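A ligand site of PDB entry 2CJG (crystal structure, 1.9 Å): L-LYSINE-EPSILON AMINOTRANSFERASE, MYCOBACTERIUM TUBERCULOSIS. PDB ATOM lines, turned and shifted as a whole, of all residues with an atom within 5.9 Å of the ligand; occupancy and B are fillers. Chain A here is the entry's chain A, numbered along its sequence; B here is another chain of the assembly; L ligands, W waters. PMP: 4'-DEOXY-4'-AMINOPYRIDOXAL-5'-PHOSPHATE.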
ATOM      1  N   VAL A  63     -30.069  -9.199 -10.614  1.00  0.00           N
ATOM      2  CA  VAL A  63     -29.693 -10.135 -11.675  1.00  0.00           C
ATOM      3  C   VAL A  63     -30.952 -10.661 -12.380  1.00  0.00           C
ATOM      4  O   VAL A  63     -31.168 -11.869 -12.443  1.00  0.00           O
ATOM      5  CB  VAL A  63     -28.769 -11.316 -11.158  1.00  0.00           C
ATOM      6  CG1 VAL A  63     -27.927 -11.876 -12.323  1.00  0.00           C
ATOM      7  CG2 VAL A  63     -27.864 -10.866  -9.953  1.00  0.00           C
ATOM      8  N   GLY A 127     -34.435 -22.281  -5.611  1.00  0.00           N
ATOM      9  CA  GLY A 127     -33.128 -22.110  -6.278  1.00  0.00           C
ATOM     10  C   GLY A 127     -33.161 -22.493  -7.760  1.00  0.00           C
ATOM     11  O   GLY A 127     -33.743 -23.529  -8.104  1.00  0.00           O
ATOM     12  N   GLY A 128     -32.519 -21.688  -8.612  1.00  0.00           N
ATOM     13  CA  GLY A 128     -32.545 -21.898 -10.071  1.00  0.00           C
ATOM     14  C   GLY A 128     -31.724 -23.125 -10.496  1.00  0.00           C
ATOM     15  O   GLY A 128     -32.123 -23.881 -11.377  1.00  0.00           O
ATOM     16  N   ALA A 129     -30.558 -23.343  -9.878  1.00  0.00           N
ATOM     17  CA  ALA A 129     -29.751 -24.540 -10.242  1.00  0.00           C
ATOM     18  C   ALA A 129     -30.551 -25.847  -9.935  1.00  0.00           C
ATOM     19  O   ALA A 129     -30.563 -26.804 -10.733  1.00  0.00           O
ATOM     20  CB  ALA A 129     -28.384 -24.503  -9.526  1.00  0.00           C
ATOM     21  N   LEU A 130     -31.243 -25.868  -8.812  1.00  0.00           N
ATOM     22  CA  LEU A 130     -32.019 -27.041  -8.427  1.00  0.00           C
ATOM     23  C   LEU A 130     -33.252 -27.236  -9.344  1.00  0.00           C
ATOM     24  O   LEU A 130     -33.651 -28.348  -9.605  1.00  0.00           O
ATOM     25  CB  LEU A 130     -32.440 -26.976  -6.952  1.00  0.00           C
ATOM     26  CG  LEU A 130     -31.815 -28.100  -6.111  1.00  0.00           C
ATOM     27  CD1 LEU A 130     -30.355 -28.297  -6.431  1.00  0.00           C
ATOM     28  CD2 LEU A 130     -32.009 -27.852  -4.621  1.00  0.00           C
ATOM     29  N   VAL A 132     -33.167 -26.585 -12.583  1.00  0.00           N
ATOM     30  CA  VAL A 132     -32.576 -27.242 -13.750  1.00  0.00           C
ATOM     31  C   VAL A 132     -32.260 -28.692 -13.409  1.00  0.00           C
ATOM     32  O   VAL A 132     -32.517 -29.588 -14.205  1.00  0.00           O
ATOM     33  CB  VAL A 132     -31.292 -26.513 -14.279  1.00  0.00           C
ATOM     34  CG1 VAL A 132     -30.590 -27.345 -15.383  1.00  0.00           C
ATOM     35  CG2 VAL A 132     -31.650 -25.090 -14.747  1.00  0.00           C
ATOM     36  N   PHE A 167     -24.907 -21.381 -19.259  1.00  0.00           N
ATOM     37  CA  PHE A 167     -24.877 -21.228 -17.804  1.00  0.00           C
ATOM     38  C   PHE A 167     -26.174 -21.794 -17.265  1.00  0.00           C
ATOM     39  O   PHE A 167     -27.234 -21.249 -17.552  1.00  0.00           O
ATOM     40  CB  PHE A 167     -24.766 -19.745 -17.368  1.00  0.00           C
ATOM     41  CG  PHE A 167     -24.535 -19.589 -15.876  1.00  0.00           C
ATOM     42  CD1 PHE A 167     -25.596 -19.687 -14.980  1.00  0.00           C
ATOM     43  CD2 PHE A 167     -23.256 -19.377 -15.375  1.00  0.00           C
ATOM     44  CE1 PHE A 167     -25.357 -19.582 -13.581  1.00  0.00           C
ATOM     45  CE2 PHE A 167     -23.025 -19.272 -13.997  1.00  0.00           C
ATOM     46  CZ  PHE A 167     -24.080 -19.381 -13.107  1.00  0.00           C
ATOM     47  N   HIS A 168     -26.073 -22.863 -16.455  1.00  0.00           N
ATOM     48  CA  HIS A 168     -27.270 -23.527 -15.892  1.00  0.00           C
ATOM     49  C   HIS A 168     -27.206 -23.618 -14.378  1.00  0.00           C
ATOM     50  O   HIS A 168     -28.097 -24.204 -13.765  1.00  0.00           O
ATOM     51  CB  HIS A 168     -27.452 -24.941 -16.495  1.00  0.00           C
ATOM     52  CG  HIS A 168     -27.699 -24.909 -17.975  1.00  0.00           C
ATOM     53  ND1 HIS A 168     -28.825 -24.320 -18.520  1.00  0.00           N
ATOM     54  CD2 HIS A 168     -26.959 -25.367 -19.015  1.00  0.00           C
ATOM     55  CE1 HIS A 168     -28.756 -24.418 -19.836  1.00  0.00           C
ATOM     56  NE2 HIS A 168     -27.640 -25.050 -20.160  1.00  0.00           N
ATOM     57  N   GLY A 169     -26.172 -23.025 -13.774  1.00  0.00           N
ATOM     58  CA  GLY A 169     -26.019 -23.074 -12.326  1.00  0.00           C
ATOM     59  C   GLY A 169     -24.699 -23.627 -11.795  1.00  0.00           C
ATOM     60  O   GLY A 169     -23.797 -24.029 -12.551  1.00  0.00           O
ATOM     61  N   ARG A 170     -24.583 -23.660 -10.466  1.00  0.00           N
ATOM     62  CA  ARG A 170     -23.340 -24.030  -9.812  1.00  0.00           C
ATOM     63  C   ARG A 170     -23.518 -25.220  -8.843  1.00  0.00           C
ATOM     64  O   ARG A 170     -22.801 -25.342  -7.828  1.00  0.00           O
ATOM     65  CB  ARG A 170     -22.812 -22.811  -9.058  1.00  0.00           C
ATOM     66  CG  ARG A 170     -22.443 -21.630  -9.948  1.00  0.00           C
ATOM     67  CD  ARG A 170     -22.112 -20.490  -8.966  1.00  0.00           C
ATOM     68  NE  ARG A 170     -21.702 -19.229  -9.558  1.00  0.00           N
ATOM     69  CZ  ARG A 170     -20.456 -18.740  -9.517  1.00  0.00           C
ATOM     70  NH1 ARG A 170     -19.458 -19.406  -8.925  1.00  0.00           N
ATOM     71  NH2 ARG A 170     -20.204 -17.544 -10.028  1.00  0.00           N
ATOM     72  N   GLU A 238     -30.416 -22.729 -22.855  1.00  0.00           N
ATOM     73  CA  GLU A 238     -31.077 -21.444 -22.717  1.00  0.00           C
ATOM     74  C   GLU A 238     -31.556 -21.009 -24.109  1.00  0.00           C
ATOM     75  O   GLU A 238     -30.792 -21.095 -25.061  1.00  0.00           O
ATOM     76  CB  GLU A 238     -30.106 -20.392 -22.190  1.00  0.00           C
ATOM     77  CG  GLU A 238     -29.472 -20.791 -20.827  1.00  0.00           C
ATOM     78  CD  GLU A 238     -28.112 -20.145 -20.692  1.00  0.00           C
ATOM     79  OE1 GLU A 238     -28.053 -18.968 -20.297  1.00  0.00           O
ATOM     80  OE2 GLU A 238     -27.134 -20.816 -21.029  1.00  0.00           O
ATOM     81  N   GLY A 242     -27.637 -16.131 -21.364  1.00  0.00           N
ATOM     82  CA  GLY A 242     -27.585 -14.908 -20.587  1.00  0.00           C
ATOM     83  C   GLY A 242     -26.180 -14.612 -20.085  1.00  0.00           C
ATOM     84  O   GLY A 242     -25.498 -13.776 -20.662  1.00  0.00           O
ATOM     85  N   GLU A 243     -25.760 -15.309 -19.037  1.00  0.00           N
ATOM     86  CA  GLU A 243     -24.429 -15.091 -18.455  1.00  0.00           C
ATOM     87  C   GLU A 243     -23.286 -15.222 -19.452  1.00  0.00           C
ATOM     88  O   GLU A 243     -22.288 -14.531 -19.321  1.00  0.00           O
ATOM     89  CB  GLU A 243     -24.148 -16.042 -17.271  1.00  0.00           C
ATOM     90  CG  GLU A 243     -25.229 -16.011 -16.199  1.00  0.00           C
ATOM     91  CD  GLU A 243     -25.423 -14.608 -15.590  1.00  0.00           C
ATOM     92  OE1 GLU A 243     -24.415 -13.992 -15.205  1.00  0.00           O
ATOM     93  OE2 GLU A 243     -26.582 -14.137 -15.465  1.00  0.00           O
ATOM     94  N   ASP A 271     -33.969 -24.046 -20.391  1.00  0.00           N
ATOM     95  CA  ASP A 271     -33.700 -23.363 -19.125  1.00  0.00           C
ATOM     96  C   ASP A 271     -34.153 -21.920 -19.317  1.00  0.00           C
ATOM     97  O   ASP A 271     -33.441 -21.115 -19.937  1.00  0.00           O
ATOM     98  CB  ASP A 271     -32.198 -23.449 -18.797  1.00  0.00           C
ATOM     99  CG  ASP A 271     -31.830 -22.712 -17.515  1.00  0.00           C
ATOM    100  OD1 ASP A 271     -32.699 -21.957 -16.972  1.00  0.00           O
ATOM    101  OD2 ASP A 271     -30.674 -22.856 -17.085  1.00  0.00           O
ATOM    102  N   GLU A 272     -35.356 -21.605 -18.839  1.00  0.00           N
ATOM    103  CA  GLU A 272     -35.900 -20.254 -18.864  1.00  0.00           C
ATOM    104  C   GLU A 272     -35.737 -19.493 -17.528  1.00  0.00           C
ATOM    105  O   GLU A 272     -36.497 -18.552 -17.214  1.00  0.00           O
ATOM    106  CB  GLU A 272     -37.379 -20.286 -19.307  1.00  0.00           C
ATOM    107  CG  GLU A 272     -37.549 -20.792 -20.760  1.00  0.00           C
ATOM    108  CD  GLU A 272     -38.079 -19.758 -21.752  1.00  0.00           C
ATOM    109  OE1 GLU A 272     -38.132 -18.523 -21.475  1.00  0.00           O
ATOM    110  OE2 GLU A 272     -38.476 -20.211 -22.831  1.00  0.00           O
ATOM    111  N   VAL A 273     -34.750 -19.881 -16.738  1.00  0.00           N
ATOM    112  CA  VAL A 273     -34.554 -19.227 -15.434  1.00  0.00           C
ATOM    113  C   VAL A 273     -34.345 -17.733 -15.642  1.00  0.00           C
ATOM    114  O   VAL A 273     -34.934 -16.911 -14.926  1.00  0.00           O
ATOM    115  CB  VAL A 273     -33.372 -19.886 -14.608  1.00  0.00           C
ATOM    116  CG1 VAL A 273     -32.900 -18.984 -13.396  1.00  0.00           C
ATOM    117  CG2 VAL A 273     -33.795 -21.286 -14.122  1.00  0.00           C
ATOM    118  N   GLN A 274     -33.531 -17.386 -16.640  1.00  0.00           N
ATOM    119  CA  GLN A 274     -33.262 -15.972 -16.919  1.00  0.00           C
ATOM    120  C   GLN A 274     -34.180 -15.327 -17.987  1.00  0.00           C
ATOM    121  O   GLN A 274     -34.447 -14.121 -17.913  1.00  0.00           O
ATOM    122  CB  GLN A 274     -31.794 -15.762 -17.289  1.00  0.00           C
ATOM    123  CG  GLN A 274     -31.451 -14.257 -17.217  1.00  0.00           C
ATOM    124  CD  GLN A 274     -29.984 -13.927 -17.162  1.00  0.00           C
ATOM    125  OE1 GLN A 274     -29.610 -12.810 -17.510  1.00  0.00           O
ATOM    126  NE2 GLN A 274     -29.144 -14.858 -16.692  1.00  0.00           N
ATOM    127  N   LYS A 300     -35.768 -17.135 -10.738  1.00  0.00           N
ATOM    128  CA  LYS A 300     -35.532 -15.684 -10.736  1.00  0.00           C
ATOM    129  C   LYS A 300     -36.827 -14.916 -10.568  1.00  0.00           C
ATOM    130  O   LYS A 300     -37.345 -14.874  -9.476  1.00  0.00           O
ATOM    131  CB  LYS A 300     -34.749 -15.236 -11.973  1.00  0.00           C
ATOM    132  CG  LYS A 300     -33.255 -15.473 -11.848  1.00  0.00           C
ATOM    133  CD  LYS A 300     -32.528 -14.868 -13.068  1.00  0.00           C
ATOM    134  CE  LYS A 300     -31.094 -15.379 -13.191  1.00  0.00           C
ATOM    135  NZ  LYS A 300     -30.207 -14.891 -12.099  1.00  0.00           N
ATOM    136  N   CYS A 305     -38.793 -21.347  -7.546  1.00  0.00           N
ATOM    137  CA  CYS A 305     -38.231 -21.940  -8.756  1.00  0.00           C
ATOM    138  C   CYS A 305     -38.914 -23.281  -9.028  1.00  0.00           C
ATOM    139  O   CYS A 305     -39.665 -23.784  -8.183  1.00  0.00           O
ATOM    140  CB  CYS A 305     -36.705 -22.095  -8.612  1.00  0.00           C
ATOM    141  SG  CYS A 305     -35.937 -20.465  -8.258  1.00  0.00           S
ATOM    142  N   ARG A 422     -25.145  -5.891 -20.442  1.00  0.00           N
ATOM    143  CA  ARG A 422     -26.544  -6.283 -20.564  1.00  0.00           C
ATOM    144  C   ARG A 422     -27.505  -5.379 -19.787  1.00  0.00           C
ATOM    145  O   ARG A 422     -27.136  -4.813 -18.729  1.00  0.00           O
ATOM    146  CB  ARG A 422     -26.721  -7.761 -20.188  1.00  0.00           C
ATOM    147  CG  ARG A 422     -26.285  -8.053 -18.788  1.00  0.00           C
ATOM    148  CD  ARG A 422     -25.523  -9.373 -18.705  1.00  0.00           C
ATOM    149  NE  ARG A 422     -26.319 -10.402 -18.126  1.00  0.00           N
ATOM    150  CZ  ARG A 422     -26.012 -11.140 -17.051  1.00  0.00           C
ATOM    151  NH1 ARG A 422     -24.887 -11.032 -16.364  1.00  0.00           N
ATOM    152  NH2 ARG A 422     -26.911 -12.030 -16.666  1.00  0.00           N
ATOM    153  N   LEU B 130     -27.941 -27.938  -1.113  1.00  0.00           N
ATOM    154  CA  LEU B 130     -26.966 -26.976  -1.626  1.00  0.00           C
ATOM    155  C   LEU B 130     -25.979 -26.519  -0.536  1.00  0.00           C
ATOM    156  O   LEU B 130     -24.827 -26.248  -0.822  1.00  0.00           O
ATOM    157  CB  LEU B 130     -27.661 -25.784  -2.287  1.00  0.00           C
ATOM    158  CG  LEU B 130     -27.384 -25.691  -3.804  1.00  0.00           C
ATOM    159  CD1 LEU B 130     -27.489 -27.035  -4.469  1.00  0.00           C
ATOM    160  CD2 LEU B 130     -28.300 -24.678  -4.467  1.00  0.00           C
ATOM    161  N   ASN B 328     -21.349 -19.227  -5.237  1.00  0.00           N
ATOM    162  CA  ASN B 328     -22.330 -18.177  -5.488  1.00  0.00           C
ATOM    163  C   ASN B 328     -23.705 -18.773  -5.741  1.00  0.00           C
ATOM    164  O   ASN B 328     -23.829 -19.959  -6.094  1.00  0.00           O
ATOM    165  CB  ASN B 328     -21.900 -17.349  -6.710  1.00  0.00           C
ATOM    166  CG  ASN B 328     -22.628 -15.984  -6.802  1.00  0.00           C
ATOM    167  OD1 ASN B 328     -22.650 -15.209  -5.846  1.00  0.00           O
ATOM    168  ND2 ASN B 328     -23.270 -15.719  -7.946  1.00  0.00           N
ATOM    169  N   SER B 329     -24.729 -17.933  -5.587  1.00  0.00           N
ATOM    170  CA  SER B 329     -26.062 -18.181  -6.149  1.00  0.00           C
ATOM    171  C   SER B 329     -26.669 -16.810  -6.431  1.00  0.00           C
ATOM    172  O   SER B 329     -26.131 -15.780  -5.958  1.00  0.00           O
ATOM    173  CB  SER B 329     -26.955 -18.984  -5.164  1.00  0.00           C
ATOM    174  OG  SER B 329     -27.278 -18.249  -3.995  1.00  0.00           O
ATOM    175  N   THR B 330     -27.756 -16.762  -7.211  1.00  0.00           N
ATOM    176  CA  THR B 330     -28.404 -15.470  -7.511  1.00  0.00           C
ATOM    177  C   THR B 330     -28.771 -14.724  -6.226  1.00  0.00           C
ATOM    178  O   THR B 330     -28.420 -13.542  -6.069  1.00  0.00           O
ATOM    179  CB  THR B 330     -29.662 -15.644  -8.424  1.00  0.00           C
ATOM    180  OG1 THR B 330     -29.241 -16.135  -9.715  1.00  0.00           O
ATOM    181  CG2 THR B 330     -30.408 -14.324  -8.589  1.00  0.00           C
ATOM    182  N   TRP B 331     -29.439 -15.408  -5.301  1.00  0.00           N
ATOM    183  CA  TRP B 331     -30.001 -14.677  -4.151  1.00  0.00           C
ATOM    184  C   TRP B 331     -29.121 -14.614  -2.895  1.00  0.00           C
ATOM    185  O   TRP B 331     -29.249 -13.660  -2.114  1.00  0.00           O
ATOM    186  CB  TRP B 331     -31.382 -15.212  -3.781  1.00  0.00           C
ATOM    187  CG  TRP B 331     -32.478 -14.772  -4.771  1.00  0.00           C
ATOM    188  CD1 TRP B 331     -32.831 -13.480  -5.110  1.00  0.00           C
ATOM    189  CD2 TRP B 331     -33.361 -15.645  -5.514  1.00  0.00           C
ATOM    190  NE1 TRP B 331     -33.883 -13.509  -6.034  1.00  0.00           N
ATOM    191  CE2 TRP B 331     -34.229 -14.820  -6.285  1.00  0.00           C
ATOM    192  CE3 TRP B 331     -33.522 -17.038  -5.573  1.00  0.00           C
ATOM    193  CZ2 TRP B 331     -35.229 -15.352  -7.126  1.00  0.00           C
ATOM    194  CZ3 TRP B 331     -34.518 -17.561  -6.411  1.00  0.00           C
ATOM    195  CH2 TRP B 331     -35.364 -16.717  -7.167  1.00  0.00           C
HETATM  196  N1  PMP L   1     -29.984 -21.008 -15.325  1.00  0.00           N
HETATM  197  C2  PMP L   1     -29.741 -19.759 -15.877  1.00  0.00           C
HETATM  198  C2A PMP L   1     -30.016 -19.496 -17.357  1.00  0.00           C
HETATM  199  C3  PMP L   1     -29.230 -18.739 -15.032  1.00  0.00           C
HETATM  200  O3  PMP L   1     -28.968 -17.512 -15.576  1.00  0.00           O
HETATM  201  C4  PMP L   1     -28.983 -18.974 -13.656  1.00  0.00           C
HETATM  202  C4A PMP L   1     -28.483 -17.880 -12.686  1.00  0.00           C
HETATM  203  N4A PMP L   1     -27.897 -16.681 -13.288  1.00  0.00           N
HETATM  204  C5  PMP L   1     -29.255 -20.247 -13.132  1.00  0.00           C
HETATM  205  C6  PMP L   1     -29.827 -21.235 -13.960  1.00  0.00           C
HETATM  206  C5A PMP L   1     -28.964 -20.577 -11.675  1.00  0.00           C
HETATM  207  O4P PMP L   1     -29.911 -19.873 -10.871  1.00  0.00           O
HETATM  208  P   PMP L   1     -29.587 -19.716  -9.274  1.00  0.00           P
HETATM  209  O1P PMP L   1     -29.054 -21.081  -8.828  1.00  0.00           O
HETATM  210  O2P PMP L   1     -30.841 -19.293  -8.534  1.00  0.00           O
HETATM  211  O3P PMP L   1     -28.453 -18.714  -9.119  1.00  0.00           O
HETATM  212  O   HOH W   1     -26.470 -21.775  -9.098  1.00  0.00           O
HETATM  213  O   HOH W   2     -25.856 -19.198  -9.879  1.00  0.00           O
HETATM  214  O   HOH W   3     -32.801 -18.579 -19.138  1.00  0.00           O
HETATM  215  O   HOH W   4     -33.218 -18.149  -9.446  1.00  0.00           O
HETATM  216  O   HOH W   5     -30.290 -18.211  -6.123  1.00  0.00           O
HETATM  217  O   HOH W   6     -27.538 -17.352 -18.046  1.00  0.00           O
HETATM  218  O   HOH W   7     -26.732 -14.886 -10.542  1.00  0.00           O
HETATM  219  O   HOH W   8     -28.785 -21.910  -6.340  1.00  0.00           O
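A nitrogen (N4A) of the ligand sits close to the side-chain amino group of Lys 300, at 3.2 Å. OG1 of Thr 330 of chain B sits at hydrogen-bond distance from O3P of the ligand (2.8 Å). An oxygen (O3) of the ligand is in hydrogen-bond range of the side-chain amide nitrogen of Gln 274. N of Ala 129 sits at hydrogen-bond distance from O1P of the ligand (2.9 Å). OE2 of Glu 243 is in salt-bridge range of N4A of the ligand (3.6 Å). The backbone NH (N) of Gly 128 lies within hydrogen-bond range of an oxygen (O2P) of the ligand. OD2 of Asp 271 sits at hydrogen-bond distance from N1 of the ligand, 2.6 Å away. An oxygen (O3P) of the ligand is in hydrogen-bond range of the backbone NH of Thr 330 of chain B (2.8 Å).
The side-chain amide oxygen (OE1) of Gln 274 sits at hydrogen-bond distance from the guanidinium group (NH2) of Arg 422 (2.9 Å). The backbone NH (N) of Gly 242 is in hydrogen-bond range of the side-chain carboxylate (OE1) of Glu 238, 3.1 Å away. ND1 of His 168 is in hydrogen-bond range of OD2 of Asp 271 (2.8 Å). The side-chain amino group (NZ) of Lys 300 is in hydrogen-bond range of the backbone carbonyl oxygen (O) of Val 63 (3.2 Å). The backbone NH (N) of Phe 167 lies within hydrogen-bond range of the side-chain carboxylate (OE2) of Glu 238 (2.9 Å). OE2 of Glu 243 is in salt-bridge range of NH2 of Arg 422. OG1 of Thr 330 of chain B lies within hydrogen-bond range of NZ of Lys 300 (2.9 Å). The side-chain carboxylate (OD1) of Asp 271 is in hydrogen-bond range of the backbone NH (N) of Val 273 (2.9 Å).
Phe 167 touches the ligand (O to C2A, 3.3 Å). O of His 168 touches C6 of the ligand, 3.4 Å away. Gly 169 touches the ligand (CA to C5A, 3.9 Å). OE1 of Glu 238 touches C2A of the ligand, at 3.6 Å. Val 273 touches the ligand (CB to N1, 3.6 Å). C of Ser 329 of chain B touches O3P of the ligand (3.7 Å). Hydrophobic or aromatic side chains that line the ligand: Ala 129, Phe 167 and Val 273.
Water W1 bridges an oxygen (O1P) of the ligand (2.7 Å) and the backbone NH (N) of Arg 170 (3.0 Å). Water W5 lies within hydrogen-bond range of O2P of the ligand (2.7 Å), N of Trp 331 of chain B (3.0 Å) and N of Thr 330 of chain B (3.1 Å). Water W4 lies within hydrogen-bond range of O2P of the ligand (2.8 Å), N of Lys 300 (3.0 Å) and SG of Cys 305 (3.8 Å). Water W6 lies within hydrogen-bond range of OE1 of Glu 238 (2.8 Å), O3 of the ligand (2.9 Å), N of Glu 243 (2.9 Å) and NE2 of Gln 274 (3.3 Å). Water W7 bridges OG1 of Thr 330 of chain B (2.9 Å) and N4A of the ligand (3.5 Å).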
